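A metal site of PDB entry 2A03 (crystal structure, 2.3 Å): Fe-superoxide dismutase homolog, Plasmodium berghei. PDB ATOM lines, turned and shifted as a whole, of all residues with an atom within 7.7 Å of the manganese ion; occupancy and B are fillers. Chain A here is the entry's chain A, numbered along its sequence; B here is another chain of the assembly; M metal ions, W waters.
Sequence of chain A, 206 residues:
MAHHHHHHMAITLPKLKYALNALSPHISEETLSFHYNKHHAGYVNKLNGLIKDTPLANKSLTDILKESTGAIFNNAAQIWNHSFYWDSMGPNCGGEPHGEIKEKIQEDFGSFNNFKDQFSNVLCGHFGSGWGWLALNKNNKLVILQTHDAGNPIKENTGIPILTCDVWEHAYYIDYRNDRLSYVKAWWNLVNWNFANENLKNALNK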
ATOM      1  N   HIS A  35     -24.243 -25.852   1.766  1.00  0.00           N
ATOM      2  CA  HIS A  35     -25.015 -26.292   0.614  1.00  0.00           C
ATOM      3  C   HIS A  35     -26.429 -26.718   1.006  1.00  0.00           C
ATOM      4  O   HIS A  35     -27.390 -26.379   0.322  1.00  0.00           O
ATOM      5  CB  HIS A  35     -24.275 -27.448  -0.078  1.00  0.00           C
ATOM      6  CG  HIS A  35     -24.611 -27.605  -1.529  1.00  0.00           C
ATOM      7  ND1 HIS A  35     -23.869 -28.414  -2.363  1.00  0.00           N
ATOM      8  CD2 HIS A  35     -25.578 -27.046  -2.297  1.00  0.00           C
ATOM      9  CE1 HIS A  35     -24.384 -28.364  -3.582  1.00  0.00           C
ATOM     10  NE2 HIS A  35     -25.418 -27.531  -3.567  1.00  0.00           N
ATOM     11  N   TYR A  36     -26.565 -27.451   2.102  1.00  0.00           N
ATOM     12  CA  TYR A  36     -27.879 -27.902   2.581  1.00  0.00           C
ATOM     13  C   TYR A  36     -28.589 -26.840   3.457  1.00  0.00           C
ATOM     14  O   TYR A  36     -29.745 -26.499   3.197  1.00  0.00           O
ATOM     15  CB  TYR A  36     -27.751 -29.215   3.330  1.00  0.00           C
ATOM     16  CG  TYR A  36     -29.046 -29.799   3.873  1.00  0.00           C
ATOM     17  CD1 TYR A  36     -30.000 -30.342   3.037  1.00  0.00           C
ATOM     18  CD2 TYR A  36     -29.311 -29.796   5.240  1.00  0.00           C
ATOM     19  CE1 TYR A  36     -31.156 -30.882   3.520  1.00  0.00           C
ATOM     20  CE2 TYR A  36     -30.494 -30.326   5.758  1.00  0.00           C
ATOM     21  CZ  TYR A  36     -31.410 -30.883   4.880  1.00  0.00           C
ATOM     22  OH  TYR A  36     -32.573 -31.433   5.343  1.00  0.00           O
ATOM     23  N   HIS A  39     -28.004 -22.915   1.096  1.00  0.00           N
ATOM     24  CA  HIS A  39     -28.512 -22.901  -0.272  1.00  0.00           C
ATOM     25  C   HIS A  39     -29.844 -23.654  -0.425  1.00  0.00           C
ATOM     26  O   HIS A  39     -30.854 -23.064  -0.855  1.00  0.00           O
ATOM     27  CB  HIS A  39     -27.465 -23.404  -1.270  1.00  0.00           C
ATOM     28  CG  HIS A  39     -26.259 -22.512  -1.390  1.00  0.00           C
ATOM     29  ND1 HIS A  39     -26.241 -21.370  -2.157  1.00  0.00           N
ATOM     30  CD2 HIS A  39     -25.015 -22.633  -0.864  1.00  0.00           C
ATOM     31  CE1 HIS A  39     -25.048 -20.808  -2.078  1.00  0.00           C
ATOM     32  NE2 HIS A  39     -24.282 -21.555  -1.295  1.00  0.00           N
ATOM     33  N   HIS A  40     -29.875 -24.934  -0.075  1.00  0.00           N
ATOM     34  CA  HIS A  40     -31.079 -25.754  -0.294  1.00  0.00           C
ATOM     35  C   HIS A  40     -32.246 -25.236   0.563  1.00  0.00           C
ATOM     36  O   HIS A  40     -33.351 -25.033   0.054  1.00  0.00           O
ATOM     37  CB  HIS A  40     -30.781 -27.231  -0.002  1.00  0.00           C
ATOM     38  CG  HIS A  40     -31.808 -28.184  -0.548  1.00  0.00           C
ATOM     39  ND1 HIS A  40     -31.682 -29.564  -0.419  1.00  0.00           N
ATOM     40  CD2 HIS A  40     -32.971 -27.983  -1.213  1.00  0.00           C
ATOM     41  CE1 HIS A  40     -32.723 -30.154  -0.977  1.00  0.00           C
ATOM     42  NE2 HIS A  40     -33.530 -29.215  -1.465  1.00  0.00           N
ATOM     43  N   TYR A  43     -33.684 -22.115  -0.914  1.00  0.00           N
ATOM     44  CA  TYR A  43     -34.579 -22.277  -2.049  1.00  0.00           C
ATOM     45  C   TYR A  43     -35.978 -22.592  -1.536  1.00  0.00           C
ATOM     46  O   TYR A  43     -36.974 -22.086  -2.054  1.00  0.00           O
ATOM     47  CB  TYR A  43     -34.104 -23.365  -3.023  1.00  0.00           C
ATOM     48  CG  TYR A  43     -32.833 -23.026  -3.815  1.00  0.00           C
ATOM     49  CD1 TYR A  43     -32.755 -21.880  -4.610  1.00  0.00           C
ATOM     50  CD2 TYR A  43     -31.742 -23.865  -3.766  1.00  0.00           C
ATOM     51  CE1 TYR A  43     -31.617 -21.583  -5.321  1.00  0.00           C
ATOM     52  CE2 TYR A  43     -30.579 -23.585  -4.468  1.00  0.00           C
ATOM     53  CZ  TYR A  43     -30.519 -22.453  -5.245  1.00  0.00           C
ATOM     54  OH  TYR A  43     -29.367 -22.203  -5.967  1.00  0.00           O
ATOM     55  N   GLN A  78     -34.763 -25.985  -8.063  1.00  0.00           N
ATOM     56  CA  GLN A  78     -33.538 -26.149  -7.276  1.00  0.00           C
ATOM     57  C   GLN A  78     -33.805 -26.971  -6.019  1.00  0.00           C
ATOM     58  O   GLN A  78     -32.923 -27.716  -5.584  1.00  0.00           O
ATOM     59  CB  GLN A  78     -32.882 -24.796  -6.927  1.00  0.00           C
ATOM     60  CG  GLN A  78     -32.155 -24.130  -8.137  1.00  0.00           C
ATOM     61  CD  GLN A  78     -30.901 -24.897  -8.570  1.00  0.00           C
ATOM     62  OE1 GLN A  78     -30.977 -25.886  -9.302  1.00  0.00           O
ATOM     63  NE2 GLN A  78     -29.733 -24.430  -8.122  1.00  0.00           N
ATOM     64  N   ASN A  81     -33.936 -30.501  -7.507  1.00  0.00           N
ATOM     65  CA  ASN A  81     -32.589 -30.860  -7.967  1.00  0.00           C
ATOM     66  C   ASN A  81     -31.668 -31.216  -6.784  1.00  0.00           C
ATOM     67  O   ASN A  81     -30.959 -32.232  -6.832  1.00  0.00           O
ATOM     68  CB  ASN A  81     -31.964 -29.742  -8.789  1.00  0.00           C
ATOM     69  CG  ASN A  81     -32.722 -29.436 -10.085  1.00  0.00           C
ATOM     70  OD1 ASN A  81     -33.499 -30.248 -10.587  1.00  0.00           O
ATOM     71  ND2 ASN A  81     -32.491 -28.219 -10.621  1.00  0.00           N
ATOM     72  N   HIS A  82     -31.661 -30.399  -5.743  1.00  0.00           N
ATOM     73  CA  HIS A  82     -30.781 -30.645  -4.595  1.00  0.00           C
ATOM     74  C   HIS A  82     -31.167 -31.875  -3.821  1.00  0.00           C
ATOM     75  O   HIS A  82     -30.299 -32.653  -3.445  1.00  0.00           O
ATOM     76  CB  HIS A  82     -30.716 -29.440  -3.668  1.00  0.00           C
ATOM     77  CG  HIS A  82     -29.860 -28.362  -4.219  1.00  0.00           C
ATOM     78  ND1 HIS A  82     -30.338 -27.424  -5.112  1.00  0.00           N
ATOM     79  CD2 HIS A  82     -28.542 -28.099  -4.051  1.00  0.00           C
ATOM     80  CE1 HIS A  82     -29.347 -26.628  -5.470  1.00  0.00           C
ATOM     81  NE2 HIS A  82     -28.245 -27.016  -4.853  1.00  0.00           N
ATOM     82  N   TYR A  85     -29.848 -34.644  -5.772  1.00  0.00           N
ATOM     83  CA  TYR A  85     -28.396 -34.681  -5.595  1.00  0.00           C
ATOM     84  C   TYR A  85     -27.987 -35.356  -4.268  1.00  0.00           C
ATOM     85  O   TYR A  85     -27.072 -36.198  -4.235  1.00  0.00           O
ATOM     86  CB  TYR A  85     -27.869 -33.232  -5.762  1.00  0.00           C
ATOM     87  CG  TYR A  85     -26.428 -32.942  -5.427  1.00  0.00           C
ATOM     88  CD1 TYR A  85     -25.391 -33.414  -6.226  1.00  0.00           C
ATOM     89  CD2 TYR A  85     -26.098 -32.135  -4.337  1.00  0.00           C
ATOM     90  CE1 TYR A  85     -24.059 -33.132  -5.923  1.00  0.00           C
ATOM     91  CE2 TYR A  85     -24.769 -31.822  -4.040  1.00  0.00           C
ATOM     92  CZ  TYR A  85     -23.760 -32.329  -4.839  1.00  0.00           C
ATOM     93  OH  TYR A  85     -22.438 -32.045  -4.539  1.00  0.00           O
ATOM     94  N   TRP A  86     -28.655 -35.037  -3.175  1.00  0.00           N
ATOM     95  CA  TRP A  86     -28.310 -35.693  -1.916  1.00  0.00           C
ATOM     96  C   TRP A  86     -28.584 -37.195  -2.019  1.00  0.00           C
ATOM     97  O   TRP A  86     -27.804 -38.014  -1.532  1.00  0.00           O
ATOM     98  CB  TRP A  86     -29.046 -35.079  -0.713  1.00  0.00           C
ATOM     99  CG  TRP A  86     -28.855 -33.589  -0.626  1.00  0.00           C
ATOM    100  CD1 TRP A  86     -29.841 -32.641  -0.576  1.00  0.00           C
ATOM    101  CD2 TRP A  86     -27.612 -32.877  -0.579  1.00  0.00           C
ATOM    102  NE1 TRP A  86     -29.289 -31.393  -0.502  1.00  0.00           N
ATOM    103  CE2 TRP A  86     -27.919 -31.501  -0.529  1.00  0.00           C
ATOM    104  CE3 TRP A  86     -26.261 -33.258  -0.592  1.00  0.00           C
ATOM    105  CZ2 TRP A  86     -26.953 -30.528  -0.494  1.00  0.00           C
ATOM    106  CZ3 TRP A  86     -25.300 -32.282  -0.538  1.00  0.00           C
ATOM    107  CH2 TRP A  86     -25.652 -30.927  -0.494  1.00  0.00           C
ATOM    108  N   GLY A 130     -24.873 -25.173 -13.308  1.00  0.00           N
ATOM    109  CA  GLY A 130     -25.647 -26.233 -13.909  1.00  0.00           C
ATOM    110  C   GLY A 130     -25.556 -27.571 -13.205  1.00  0.00           C
ATOM    111  O   GLY A 130     -25.143 -27.664 -12.032  1.00  0.00           O
ATOM    112  N   TRP A 131     -25.983 -28.591 -13.945  1.00  0.00           N
ATOM    113  CA  TRP A 131     -26.131 -29.936 -13.476  1.00  0.00           C
ATOM    114  C   TRP A 131     -25.772 -30.909 -14.604  1.00  0.00           C
ATOM    115  O   TRP A 131     -26.023 -30.648 -15.777  1.00  0.00           O
ATOM    116  CB  TRP A 131     -27.600 -30.185 -13.090  1.00  0.00           C
ATOM    117  CG  TRP A 131     -28.121 -29.263 -12.030  1.00  0.00           C
ATOM    118  CD1 TRP A 131     -28.654 -28.030 -12.213  1.00  0.00           C
ATOM    119  CD2 TRP A 131     -28.155 -29.518 -10.629  1.00  0.00           C
ATOM    120  NE1 TRP A 131     -29.004 -27.477 -11.014  1.00  0.00           N
ATOM    121  CE2 TRP A 131     -28.709 -28.373 -10.020  1.00  0.00           C
ATOM    122  CE3 TRP A 131     -27.767 -30.588  -9.828  1.00  0.00           C
ATOM    123  CZ2 TRP A 131     -28.894 -28.274  -8.639  1.00  0.00           C
ATOM    124  CZ3 TRP A 131     -27.931 -30.495  -8.452  1.00  0.00           C
ATOM    125  CH2 TRP A 131     -28.495 -29.340  -7.878  1.00  0.00           C
ATOM    126  N   ASP A 166     -24.300 -31.840  -8.973  1.00  0.00           N
ATOM    127  CA  ASP A 166     -24.320 -30.372  -8.989  1.00  0.00           C
ATOM    128  C   ASP A 166     -22.950 -29.835  -9.406  1.00  0.00           C
ATOM    129  O   ASP A 166     -21.939 -30.160  -8.787  1.00  0.00           O
ATOM    130  CB  ASP A 166     -24.678 -29.910  -7.572  1.00  0.00           C
ATOM    131  CG  ASP A 166     -25.078 -28.436  -7.483  1.00  0.00           C
ATOM    132  OD1 ASP A 166     -25.015 -27.698  -8.493  1.00  0.00           O
ATOM    133  OD2 ASP A 166     -25.477 -28.012  -6.369  1.00  0.00           O
ATOM    134  N   VAL A 167     -22.899 -28.972 -10.426  1.00  0.00           N
ATOM    135  CA  VAL A 167     -21.680 -28.246 -10.746  1.00  0.00           C
ATOM    136  C   VAL A 167     -21.784 -26.714 -10.614  1.00  0.00           C
ATOM    137  O   VAL A 167     -20.920 -26.013 -11.099  1.00  0.00           O
ATOM    138  CB  VAL A 167     -21.085 -28.648 -12.133  1.00  0.00           C
ATOM    139  CG1 VAL A 167     -20.777 -30.169 -12.183  1.00  0.00           C
ATOM    140  CG2 VAL A 167     -21.984 -28.231 -13.268  1.00  0.00           C
ATOM    141  N   TRP A 168     -22.806 -26.204  -9.931  1.00  0.00           N
ATOM    142  CA  TRP A 168     -22.716 -24.807  -9.419  1.00  0.00           C
ATOM    143  C   TRP A 168     -21.434 -24.701  -8.586  1.00  0.00           C
ATOM    144  O   TRP A 168     -21.088 -25.632  -7.835  1.00  0.00           O
ATOM    145  CB  TRP A 168     -23.893 -24.437  -8.522  1.00  0.00           C
ATOM    146  CG  TRP A 168     -25.192 -24.209  -9.251  1.00  0.00           C
ATOM    147  CD1 TRP A 168     -25.850 -25.080 -10.081  1.00  0.00           C
ATOM    148  CD2 TRP A 168     -26.001 -23.025  -9.207  1.00  0.00           C
ATOM    149  NE1 TRP A 168     -26.998 -24.503 -10.559  1.00  0.00           N
ATOM    150  CE2 TRP A 168     -27.119 -23.240 -10.031  1.00  0.00           C
ATOM    151  CE3 TRP A 168     -25.876 -21.797  -8.550  1.00  0.00           C
ATOM    152  CZ2 TRP A 168     -28.099 -22.284 -10.218  1.00  0.00           C
ATOM    153  CZ3 TRP A 168     -26.854 -20.861  -8.723  1.00  0.00           C
ATOM    154  CH2 TRP A 168     -27.954 -21.102  -9.560  1.00  0.00           C
ATOM    155  N   GLU A 169     -20.742 -23.573  -8.673  1.00  0.00           N
ATOM    156  CA  GLU A 169     -19.473 -23.402  -7.945  1.00  0.00           C
ATOM    157  C   GLU A 169     -19.610 -23.663  -6.431  1.00  0.00           C
ATOM    158  O   GLU A 169     -18.657 -24.149  -5.800  1.00  0.00           O
ATOM    159  CB  GLU A 169     -18.839 -22.030  -8.233  1.00  0.00           C
ATOM    160  CG  GLU A 169     -18.215 -21.983  -9.604  1.00  0.00           C
ATOM    161  CD  GLU A 169     -17.716 -20.606 -10.065  1.00  0.00           C
ATOM    162  OE1 GLU A 169     -18.304 -19.559  -9.708  1.00  0.00           O
ATOM    163  OE2 GLU A 169     -16.731 -20.600 -10.839  1.00  0.00           O
ATOM    164  N   HIS A 170     -20.771 -23.378  -5.849  1.00  0.00           N
ATOM    165  CA  HIS A 170     -20.985 -23.534  -4.396  1.00  0.00           C
ATOM    166  C   HIS A 170     -20.941 -24.988  -3.944  1.00  0.00           C
ATOM    167  O   HIS A 170     -20.763 -25.271  -2.752  1.00  0.00           O
ATOM    168  CB  HIS A 170     -22.303 -22.871  -3.922  1.00  0.00           C
ATOM    169  CG  HIS A 170     -23.560 -23.501  -4.448  1.00  0.00           C
ATOM    170  ND1 HIS A 170     -24.510 -22.796  -5.160  1.00  0.00           N
ATOM    171  CD2 HIS A 170     -24.053 -24.763  -4.301  1.00  0.00           C
ATOM    172  CE1 HIS A 170     -25.511 -23.611  -5.472  1.00  0.00           C
ATOM    173  NE2 HIS A 170     -25.259 -24.809  -4.961  1.00  0.00           N
ATOM    174  N   ALA A 171     -21.131 -25.907  -4.886  1.00  0.00           N
ATOM    175  CA  ALA A 171     -21.083 -27.313  -4.584  1.00  0.00           C
ATOM    176  C   ALA A 171     -19.675 -27.746  -4.226  1.00  0.00           C
ATOM    177  O   ALA A 171     -19.501 -28.743  -3.522  1.00  0.00           O
ATOM    178  CB  ALA A 171     -21.603 -28.147  -5.782  1.00  0.00           C
ATOM    179  N   TYR A 172     -18.667 -27.006  -4.707  1.00  0.00           N
ATOM    180  CA  TYR A 172     -17.273 -27.422  -4.540  1.00  0.00           C
ATOM    181  C   TYR A 172     -16.258 -26.356  -4.148  1.00  0.00           C
ATOM    182  O   TYR A 172     -15.129 -26.682  -3.802  1.00  0.00           O
ATOM    183  CB  TYR A 172     -16.795 -28.146  -5.813  1.00  0.00           C
ATOM    184  CG  TYR A 172     -16.781 -27.297  -7.085  1.00  0.00           C
ATOM    185  CD1 TYR A 172     -15.680 -26.493  -7.411  1.00  0.00           C
ATOM    186  CD2 TYR A 172     -17.860 -27.341  -7.966  1.00  0.00           C
ATOM    187  CE1 TYR A 172     -15.690 -25.731  -8.573  1.00  0.00           C
ATOM    188  CE2 TYR A 172     -17.872 -26.589  -9.128  1.00  0.00           C
ATOM    189  CZ  TYR A 172     -16.778 -25.803  -9.442  1.00  0.00           C
ATOM    190  OH  TYR A 172     -16.804 -25.068 -10.604  1.00  0.00           O
ATOM    191  N   TYR A 183     -13.125 -32.169  -7.648  1.00  0.00           N
ATOM    192  CA  TYR A 183     -14.460 -32.386  -7.135  1.00  0.00           C
ATOM    193  C   TYR A 183     -15.147 -33.552  -7.888  1.00  0.00           C
ATOM    194  O   TYR A 183     -15.700 -34.480  -7.285  1.00  0.00           O
ATOM    195  CB  TYR A 183     -15.272 -31.102  -7.251  1.00  0.00           C
ATOM    196  CG  TYR A 183     -16.763 -31.289  -7.156  1.00  0.00           C
ATOM    197  CD1 TYR A 183     -17.368 -31.646  -5.964  1.00  0.00           C
ATOM    198  CD2 TYR A 183     -17.575 -31.076  -8.265  1.00  0.00           C
ATOM    199  CE1 TYR A 183     -18.760 -31.815  -5.872  1.00  0.00           C
ATOM    200  CE2 TYR A 183     -18.967 -31.246  -8.173  1.00  0.00           C
ATOM    201  CZ  TYR A 183     -19.553 -31.607  -6.976  1.00  0.00           C
ATOM    202  OH  TYR A 183     -20.919 -31.751  -6.882  1.00  0.00           O
ATOM    203  N   GLU B 169     -20.268 -17.098  -8.272  1.00  0.00           N
ATOM    204  CA  GLU B 169     -20.004 -17.474  -6.864  1.00  0.00           C
ATOM    205  C   GLU B 169     -18.514 -17.431  -6.515  1.00  0.00           C
ATOM    206  O   GLU B 169     -18.148 -17.063  -5.396  1.00  0.00           O
ATOM    207  CB  GLU B 169     -20.637 -18.842  -6.535  1.00  0.00           C
ATOM    208  CG  GLU B 169     -22.139 -18.738  -6.443  1.00  0.00           C
ATOM    209  CD  GLU B 169     -22.877 -20.072  -6.347  1.00  0.00           C
ATOM    210  OE1 GLU B 169     -22.436 -21.038  -6.984  1.00  0.00           O
ATOM    211  OE2 GLU B 169     -23.928 -20.121  -5.643  1.00  0.00           O
HETATM  212 MN    MN M   1     -26.265 -26.638  -5.326  1.00  0.00          MN
HETATM  213  O   HOH W   1     -27.105 -25.841  -7.328  1.00  0.00           O
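The backbone NH (N) of His 40 lies within hydrogen-bond range of the backbone carbonyl oxygen (O) of His 35, 2.9 Å away.
OD1 of Asp 166 is in hydrogen-bond range of N of Trp 168.
The indole nitrogen (NE1) of Trp 86 lies close to the backbone carbonyl oxygen (O) of His 82, at 3.4 Å.
The backbone carbonyl oxygen of Asp 166 sits at hydrogen-bond distance from the side-chain hydroxyl of Tyr 183 (2.7 Å).
A ring nitrogen (ND1) of His 82 is in hydrogen-bond range of the backbone carbonyl oxygen of Gln 78 (2.6 Å).
A ring nitrogen (ND1) of His 170 lies within hydrogen-bond range of the side-chain carboxylate (OE2) of Glu 169 of chain B, at 2.8 Å.
Water W1 lies within hydrogen-bond range of the side-chain carboxylate of Asp 166 (3.0 Å), the side-chain amide nitrogen of Gln 78 (3.1 Å) and the indole nitrogen of Trp 168 (3.5 Å).
Within 4 Å of the manganese ion: His 35, His 82, Asp 166 and His 170.
The manganese ion is bound by OD2 of Asp 166, NE2 of His 82, NE2 of His 170, NE2 of His 35 and water W1.
The manganese ion has five donor atoms within binding distance.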
